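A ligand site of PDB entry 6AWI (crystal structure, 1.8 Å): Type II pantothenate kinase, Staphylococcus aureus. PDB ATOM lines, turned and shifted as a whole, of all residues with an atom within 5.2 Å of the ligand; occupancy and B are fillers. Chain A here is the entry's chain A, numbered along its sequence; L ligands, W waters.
The side-chain amino group of Lys 13 is in salt-bridge range of an oxygen (O5) of the ligand, 2.7 Å away.
An oxygen (O1) of the ligand sits at hydrogen-bond distance from the backbone NH of Thr 99, 3.1 Å away.
The side-chain hydroxyl (OG1) of Thr 99 is in hydrogen-bond range of an oxygen (O1) of the ligand.
N of Ser 225 is in hydrogen-bond range of O4 of the ligand, 2.8 Å away.
OG of Ser 225 lies within hydrogen-bond range of O5 of the ligand, at 2.8 Å.
N of Thr 10 lies within hydrogen-bond range of O2 of the ligand (2.9 Å).
N of Leu 11 lies within hydrogen-bond range of O2 of the ligand, 2.9 Å away.
The side-chain amide oxygen (OE1) of Gln 125 is in hydrogen-bond range of an oxygen (O9) of the ligand (2.9 Å).
An oxygen (O10) of the ligand lies close to the backbone carbonyl oxygen (O) of Gly 121, 3.2 Å away.
The backbone NH (N) of Gly 9 sits at hydrogen-bond distance from an oxygen (O2) of the ligand (3.3 Å).
N of Ser 226 lies within hydrogen-bond range of O8 of the ligand (3.4 Å).
N of Gly 122 is in hydrogen-bond range of O9 of the ligand (3.4 Å).
The side-chain amino group of Lys 13 is in hydrogen-bond range of the backbone carbonyl oxygen of Leu 11, at 3.0 Å.
The side-chain hydroxyl (OG1) of Thr 99 is in hydrogen-bond range of the side-chain hydroxyl (OG1) of Thr 10.
O of Thr 99 lies within hydrogen-bond range of N of Gly 122, at 2.9 Å.
The backbone NH (N) of Gly 121 lies within hydrogen-bond range of the backbone carbonyl oxygen (O) of Gly 98 (2.8 Å).
The backbone NH (N) of Gly 121 sits close to the side-chain hydroxyl (OG) of Ser 226, at 3.3 Å.
The backbone carbonyl oxygen (O) of His 228 sits at hydrogen-bond distance from the side-chain hydroxyl (OH) of Tyr 137 (2.8 Å).
The backbone carbonyl oxygen of Gly 98 lies within hydrogen-bond range of the side-chain hydroxyl of Ser 226.
The backbone carbonyl oxygen (O) of Val 97 sits at hydrogen-bond distance from the side-chain hydroxyl (OG) of Ser 226 (2.8 Å).
Gly 8 touches the ligand.
Leu 28 touches the ligand (CD2 to N4, 3.998 Å).
Gly 98 touches the ligand (CA to O6, 3.3 Å).
Tyr 137 touches the ligand.
Gly 224 touches the ligand (CA to O4, 3.5 Å).
Hydrophobic or aromatic side chains within 4 Å of the ligand: Leu 11, Leu 28 and Tyr 137.
Of the 23 residues printed, 15 come within 4 Å of the ligand.
The nearest printed residue that does not touch the ligand is Val 97 (4.02 Å).
Water W1 bridges an oxygen (O1) of the ligand (2.5 Å) and the backbone NH (N) of Gly 9 (3.2 Å).
Water W4 lies within hydrogen-bond range of O4 of the ligand (2.8 Å) and O of Ala 255 (2.8 Å).
Water W3 lies within hydrogen-bond range of the side-chain carboxylate of Asp 6, an oxygen (O3) of the ligand and the side-chain amino group of Lys 13.
Water W5 lies within hydrogen-bond range of the side-chain amide oxygen of Asn 96 and an oxygen (O4) of the ligand.
Water W6 lies within hydrogen-bond range of N of Gly 100, O1 of the ligand and N of Thr 99.
Water W7 bridges OD1 of Asp 6 (2.4 Å) and O3 of the ligand (3.2 Å).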
ATOM      1  N   ASP A   6       0.433 -20.551  11.057  1.00  0.00           N
ATOM      2  CA  ASP A   6       1.190 -19.453  10.481  1.00  0.00           C
ATOM      3  C   ASP A   6       1.516 -18.504  11.621  1.00  0.00           C
ATOM      4  O   ASP A   6       0.704 -17.690  12.003  1.00  0.00           O
ATOM      5  CB  ASP A   6       0.350 -18.754   9.414  1.00  0.00           C
ATOM      6  CG  ASP A   6       1.106 -17.665   8.705  1.00  0.00           C
ATOM      7  OD1 ASP A   6       2.292 -17.415   9.095  1.00  0.00           O
ATOM      8  OD2 ASP A   6       0.539 -16.977   7.739  1.00  0.00           O
ATOM      9  N   GLY A   8       3.314 -15.566  12.720  1.00  0.00           N
ATOM     10  CA  GLY A   8       3.874 -14.353  12.198  1.00  0.00           C
ATOM     11  C   GLY A   8       4.502 -13.441  13.215  1.00  0.00           C
ATOM     12  O   GLY A   8       4.665 -13.808  14.373  1.00  0.00           O
ATOM     13  N   GLY A   9       4.871 -12.259  12.784  1.00  0.00           N
ATOM     14  CA  GLY A   9       5.536 -11.333  13.698  1.00  0.00           C
ATOM     15  C   GLY A   9       4.650 -10.777  14.818  1.00  0.00           C
ATOM     16  O   GLY A   9       5.142 -10.372  15.921  1.00  0.00           O
ATOM     17  N   THR A  10       3.351 -10.714  14.547  1.00  0.00           N
ATOM     18  CA  THR A  10       2.392 -10.171  15.501  1.00  0.00           C
ATOM     19  C   THR A  10       1.279 -11.207  15.955  1.00  0.00           C
ATOM     20  O   THR A  10       0.942 -11.273  17.140  1.00  0.00           O
ATOM     21  CB  THR A  10       1.702  -8.918  14.914  1.00  0.00           C
ATOM     22  OG1 THR A  10       2.724  -7.981  14.484  1.00  0.00           O
ATOM     23  CG2 THR A  10       0.771  -8.267  16.010  1.00  0.00           C
ATOM     24  N   LEU A  11       0.730 -11.943  15.020  1.00  0.00           N
ATOM     25  CA  LEU A  11      -0.356 -12.883  15.285  1.00  0.00           C
ATOM     26  C   LEU A  11       0.065 -14.284  14.877  1.00  0.00           C
ATOM     27  O   LEU A  11       0.798 -14.473  13.878  1.00  0.00           O
ATOM     28  CB  LEU A  11      -1.622 -12.478  14.543  1.00  0.00           C
ATOM     29  CG  LEU A  11      -2.181 -11.144  14.994  1.00  0.00           C
ATOM     30  CD1 LEU A  11      -3.403 -10.759  14.162  1.00  0.00           C
ATOM     31  CD2 LEU A  11      -2.487 -11.039  16.479  1.00  0.00           C
ATOM     32  N   LYS A  13      -1.718 -17.628  13.676  1.00  0.00           N
ATOM     33  CA  LYS A  13      -2.967 -18.095  13.044  1.00  0.00           C
ATOM     34  C   LYS A  13      -2.943 -19.582  13.003  1.00  0.00           C
ATOM     35  O   LYS A  13      -1.988 -20.202  12.515  1.00  0.00           O
ATOM     36  CB  LYS A  13      -3.119 -17.544  11.658  1.00  0.00           C
ATOM     37  CG  LYS A  13      -3.581 -16.091  11.558  1.00  0.00           C
ATOM     38  CD  LYS A  13      -2.517 -15.055  11.883  1.00  0.00           C
ATOM     39  CE  LYS A  13      -1.351 -15.049  10.872  1.00  0.00           C
ATOM     40  NZ  LYS A  13      -0.419 -14.020  11.221  1.00  0.00           N
ATOM     41  N   LEU A  28      -1.920 -14.165  20.080  1.00  0.00           N
ATOM     42  CA  LEU A  28      -0.814 -13.224  19.972  1.00  0.00           C
ATOM     43  C   LEU A  28       0.537 -13.913  19.898  1.00  0.00           C
ATOM     44  O   LEU A  28       0.799 -14.909  20.633  1.00  0.00           O
ATOM     45  CB  LEU A  28      -0.819 -12.233  21.106  1.00  0.00           C
ATOM     46  CG  LEU A  28      -2.150 -11.533  21.233  1.00  0.00           C
ATOM     47  CD1 LEU A  28      -2.146 -10.782  22.564  1.00  0.00           C
ATOM     48  CD2 LEU A  28      -2.407 -10.600  20.061  1.00  0.00           C
ATOM     49  N   THR A  29       1.407 -13.379  19.017  1.00  0.00           N
ATOM     50  CA  THR A  29       2.829 -13.821  19.028  1.00  0.00           C
ATOM     51  C   THR A  29       3.475 -13.641  20.345  1.00  0.00           C
ATOM     52  O   THR A  29       4.227 -14.491  20.801  1.00  0.00           O
ATOM     53  CB  THR A  29       3.633 -13.308  17.826  1.00  0.00           C
ATOM     54  OG1 THR A  29       2.956 -13.758  16.670  1.00  0.00           O
ATOM     55  CG2 THR A  29       5.013 -13.946  17.798  1.00  0.00           C
ATOM     56  N   ASN A  96      -0.243  -9.318   0.795  1.00  0.00           N
ATOM     57  CA  ASN A  96      -0.372  -9.805   2.131  1.00  0.00           C
ATOM     58  C   ASN A  96       0.036  -8.750   3.166  1.00  0.00           C
ATOM     59  O   ASN A  96       1.241  -8.518   3.413  1.00  0.00           O
ATOM     60  CB  ASN A  96       0.421 -11.150   2.229  1.00  0.00           C
ATOM     61  CG  ASN A  96       0.166 -11.903   3.502  1.00  0.00           C
ATOM     62  OD1 ASN A  96      -0.634 -11.507   4.332  1.00  0.00           O
ATOM     63  ND2 ASN A  96       0.877 -13.009   3.678  1.00  0.00           N
ATOM     64  N   VAL A  97      -0.992  -8.103   3.777  1.00  0.00           N
ATOM     65  CA  VAL A  97      -0.802  -6.937   4.582  1.00  0.00           C
ATOM     66  C   VAL A  97      -0.819  -7.370   6.031  1.00  0.00           C
ATOM     67  O   VAL A  97      -1.832  -7.389   6.696  1.00  0.00           O
ATOM     68  CB  VAL A  97      -1.862  -5.848   4.275  1.00  0.00           C
ATOM     69  CG1 VAL A  97      -1.512  -4.576   5.031  1.00  0.00           C
ATOM     70  CG2 VAL A  97      -1.906  -5.632   2.805  1.00  0.00           C
ATOM     71  N   GLY A  98       0.339  -7.759   6.443  1.00  0.00           N
ATOM     72  CA  GLY A  98       0.570  -8.201   7.811  1.00  0.00           C
ATOM     73  C   GLY A  98       1.280  -7.165   8.675  1.00  0.00           C
ATOM     74  O   GLY A  98       1.045  -6.001   8.559  1.00  0.00           O
ATOM     75  N   THR A  99       2.148  -7.646   9.588  1.00  0.00           N
ATOM     76  CA  THR A  99       3.000  -6.779  10.311  1.00  0.00           C
ATOM     77  C   THR A  99       3.713  -5.859   9.283  1.00  0.00           C
ATOM     78  O   THR A  99       3.791  -4.619   9.490  1.00  0.00           O
ATOM     79  CB  THR A  99       4.046  -7.592  11.044  1.00  0.00           C
ATOM     80  OG1 THR A  99       3.368  -8.467  11.979  1.00  0.00           O
ATOM     81  CG2 THR A  99       4.922  -6.625  11.793  1.00  0.00           C
ATOM     82  N   GLY A 100       4.136  -6.464   8.162  1.00  0.00           N
ATOM     83  CA  GLY A 100       4.620  -5.797   7.002  1.00  0.00           C
ATOM     84  C   GLY A 100       3.870  -6.316   5.765  1.00  0.00           C
ATOM     85  O   GLY A 100       3.090  -7.248   5.876  1.00  0.00           O
ATOM     86  N   GLY A 121       0.367  -3.343   8.914  1.00  0.00           N
ATOM     87  CA  GLY A 121      -0.266  -3.256  10.229  1.00  0.00           C
ATOM     88  C   GLY A 121       0.642  -2.920  11.396  1.00  0.00           C
ATOM     89  O   GLY A 121       0.203  -2.396  12.404  1.00  0.00           O
ATOM     90  N   GLY A 122       1.923  -3.269  11.280  1.00  0.00           N
ATOM     91  CA  GLY A 122       2.899  -2.946  12.323  1.00  0.00           C
ATOM     92  C   GLY A 122       3.123  -1.449  12.345  1.00  0.00           C
ATOM     93  O   GLY A 122       3.308  -0.809  13.400  1.00  0.00           O
ATOM     94  N   ILE A 124       0.720   0.709  11.423  1.00  0.00           N
ATOM     95  CA  ILE A 124      -0.516   1.199  11.992  1.00  0.00           C
ATOM     96  C   ILE A 124      -0.462   1.190  13.476  1.00  0.00           C
ATOM     97  O   ILE A 124      -0.783   2.170  14.151  1.00  0.00           O
ATOM     98  CB  ILE A 124      -1.709   0.412  11.446  1.00  0.00           C
ATOM     99  CG1 ILE A 124      -1.869   0.737   9.983  1.00  0.00           C
ATOM    100  CG2 ILE A 124      -2.986   0.743  12.228  1.00  0.00           C
ATOM    101  CD1 ILE A 124      -2.871  -0.131   9.225  1.00  0.00           C
ATOM    102  N   GLN A 125      -0.030   0.055  14.034  1.00  0.00           N
ATOM    103  CA  GLN A 125       0.139  -0.035  15.504  1.00  0.00           C
ATOM    104  C   GLN A 125       1.254   0.856  16.110  1.00  0.00           C
ATOM    105  O   GLN A 125       1.030   1.522  17.093  1.00  0.00           O
ATOM    106  CB  GLN A 125       0.324  -1.489  15.944  1.00  0.00           C
ATOM    107  CG  GLN A 125      -0.834  -2.434  15.668  1.00  0.00           C
ATOM    108  CD  GLN A 125      -0.473  -3.759  16.220  1.00  0.00           C
ATOM    109  OE1 GLN A 125       0.151  -4.618  15.565  1.00  0.00           O
ATOM    110  NE2 GLN A 125      -0.726  -3.897  17.476  1.00  0.00           N
ATOM    111  N   TYR A 137      -5.071  -2.684  20.320  1.00  0.00           N
ATOM    112  CA  TYR A 137      -5.466  -2.633  18.888  1.00  0.00           C
ATOM    113  C   TYR A 137      -6.957  -2.302  18.584  1.00  0.00           C
ATOM    114  O   TYR A 137      -7.230  -1.540  17.640  1.00  0.00           O
ATOM    115  CB  TYR A 137      -5.158  -3.985  18.230  1.00  0.00           C
ATOM    116  CG  TYR A 137      -5.524  -4.052  16.787  1.00  0.00           C
ATOM    117  CD1 TYR A 137      -4.715  -3.513  15.839  1.00  0.00           C
ATOM    118  CD2 TYR A 137      -6.679  -4.720  16.365  1.00  0.00           C
ATOM    119  CE1 TYR A 137      -5.069  -3.562  14.511  1.00  0.00           C
ATOM    120  CE2 TYR A 137      -7.042  -4.818  15.022  1.00  0.00           C
ATOM    121  CZ  TYR A 137      -6.211  -4.233  14.090  1.00  0.00           C
ATOM    122  OH  TYR A 137      -6.524  -4.260  12.758  1.00  0.00           O
ATOM    123  N   GLY A 224      -4.490 -10.635   4.982  1.00  0.00           N
ATOM    124  CA  GLY A 224      -3.738 -10.240   6.167  1.00  0.00           C
ATOM    125  C   GLY A 224      -4.628  -9.746   7.272  1.00  0.00           C
ATOM    126  O   GLY A 224      -5.716  -9.240   7.030  1.00  0.00           O
ATOM    127  N   SER A 225      -4.179  -9.873   8.496  1.00  0.00           N
ATOM    128  CA  SER A 225      -4.985  -9.518   9.571  1.00  0.00           C
ATOM    129  C   SER A 225      -5.224  -7.994   9.715  1.00  0.00           C
ATOM    130  O   SER A 225      -6.020  -7.584  10.522  1.00  0.00           O
ATOM    131  CB  SER A 225      -4.411  -9.985  10.897  1.00  0.00           C
ATOM    132  OG  SER A 225      -4.248 -11.414  10.884  1.00  0.00           O
ATOM    133  N   SER A 226      -4.455  -7.177   9.013  1.00  0.00           N
ATOM    134  CA  SER A 226      -4.539  -5.742   9.163  1.00  0.00           C
ATOM    135  C   SER A 226      -5.925  -5.259   8.770  1.00  0.00           C
ATOM    136  O   SER A 226      -6.233  -4.152   9.121  1.00  0.00           O
ATOM    137  CB  SER A 226      -3.465  -5.002   8.287  1.00  0.00           C
ATOM    138  OG  SER A 226      -2.187  -5.420   8.643  1.00  0.00           O
ATOM    139  N   HIS A 228      -8.732  -6.596   9.761  1.00  0.00           N
ATOM    140  CA  HIS A 228      -9.667  -6.932  10.798  1.00  0.00           C
ATOM    141  C   HIS A 228      -9.980  -5.742  11.666  1.00  0.00           C
ATOM    142  O   HIS A 228      -9.103  -5.104  12.198  1.00  0.00           O
ATOM    143  CB  HIS A 228      -9.063  -8.016  11.697  1.00  0.00           C
ATOM    144  CG  HIS A 228      -8.935  -9.334  11.011  1.00  0.00           C
ATOM    145  ND1 HIS A 228      -8.379 -10.454  11.609  1.00  0.00           N
ATOM    146  CD2 HIS A 228      -9.260  -9.706   9.746  1.00  0.00           C
ATOM    147  CE1 HIS A 228      -8.409 -11.470  10.758  1.00  0.00           C
ATOM    148  NE2 HIS A 228      -8.926 -11.031   9.609  1.00  0.00           N
ATOM    149  N   ALA A 255      -6.906 -13.931   6.289  1.00  0.00           N
ATOM    150  CA  ALA A 255      -5.762 -13.866   7.206  1.00  0.00           C
ATOM    151  C   ALA A 255      -5.170 -15.204   7.579  1.00  0.00           C
ATOM    152  O   ALA A 255      -4.071 -15.214   8.128  1.00  0.00           O
ATOM    153  CB  ALA A 255      -6.093 -13.115   8.470  1.00  0.00           C
HETATM  154  P1  LIG L   1       1.787 -11.378  10.825  1.00  0.00           P
HETATM  155  O1  LIG L   1       2.965 -10.585  10.340  1.00  0.00           O
HETATM  156  O2  LIG L   1       1.688 -11.508  12.308  1.00  0.00           O
HETATM  157  O3  LIG L   1       1.643 -12.668  10.068  1.00  0.00           O
HETATM  158  P2  LIG L   1      -1.005 -10.610  10.233  1.00  0.00           P
HETATM  159  O4  LIG L   1      -1.499 -10.771   8.835  1.00  0.00           O
HETATM  160  O5  LIG L   1      -1.482 -11.536  11.289  1.00  0.00           O
HETATM  161  O6  LIG L   1       0.616 -10.447  10.271  1.00  0.00           O
HETATM  162  O7  LIG L   1      -1.321  -9.066  10.529  1.00  0.00           O
HETATM  163  C1  LIG L   1      -0.823  -8.387  11.672  1.00  0.00           C
HETATM  164  C2  LIG L   1      -1.583  -7.114  11.914  1.00  0.00           C
HETATM  165  O8  LIG L   1      -2.964  -7.295  12.032  1.00  0.00           O
HETATM  166  C3  LIG L   1      -1.279  -6.286  13.151  1.00  0.00           C
HETATM  167  O9  LIG L   1      -0.008  -5.609  12.820  1.00  0.00           O
HETATM  168  C4  LIG L   1      -2.479  -5.391  13.280  1.00  0.00           C
HETATM  169  O10 LIG L   1      -2.386  -4.282  12.383  1.00  0.00           O
HETATM  170  C5  LIG L   1      -3.612  -6.276  12.760  1.00  0.00           C
HETATM  171  N1  LIG L   1      -4.390  -6.942  13.877  1.00  0.00           N
HETATM  172  C6  LIG L   1      -5.565  -7.546  13.654  1.00  0.00           C
HETATM  173  N2  LIG L   1      -6.078  -8.067  14.782  1.00  0.00           N
HETATM  174  C7  LIG L   1      -5.190  -7.856  15.739  1.00  0.00           C
HETATM  175  C8  LIG L   1      -5.085  -8.105  17.173  1.00  0.00           C
HETATM  176  N3  LIG L   1      -6.072  -8.791  17.836  1.00  0.00           N
HETATM  177  N4  LIG L   1      -4.014  -7.699  17.829  1.00  0.00           N
HETATM  178  C9  LIG L   1      -2.986  -7.076  17.251  1.00  0.00           C
HETATM  179  N5  LIG L   1      -3.066  -6.810  15.951  1.00  0.00           N
HETATM  180  C10 LIG L   1      -4.086  -7.140  15.150  1.00  0.00           C
HETATM  181  O   HOH W   1       5.105 -11.714   9.617  1.00  0.00           O
HETATM  182  O   HOH W   2       2.823 -12.927   7.369  1.00  0.00           O
HETATM  183  O   HOH W   3       0.245 -14.387   8.219  1.00  0.00           O
HETATM  184  O   HOH W   4      -2.026 -13.328   7.944  1.00  0.00           O
HETATM  185  O   HOH W   5       0.507 -11.653   6.815  1.00  0.00           O
HETATM  186  O   HOH W   6       4.258  -9.401   7.660  1.00  0.00           O
HETATM  187  O   HOH W   7       3.186 -15.182   8.762  1.00  0.00           O
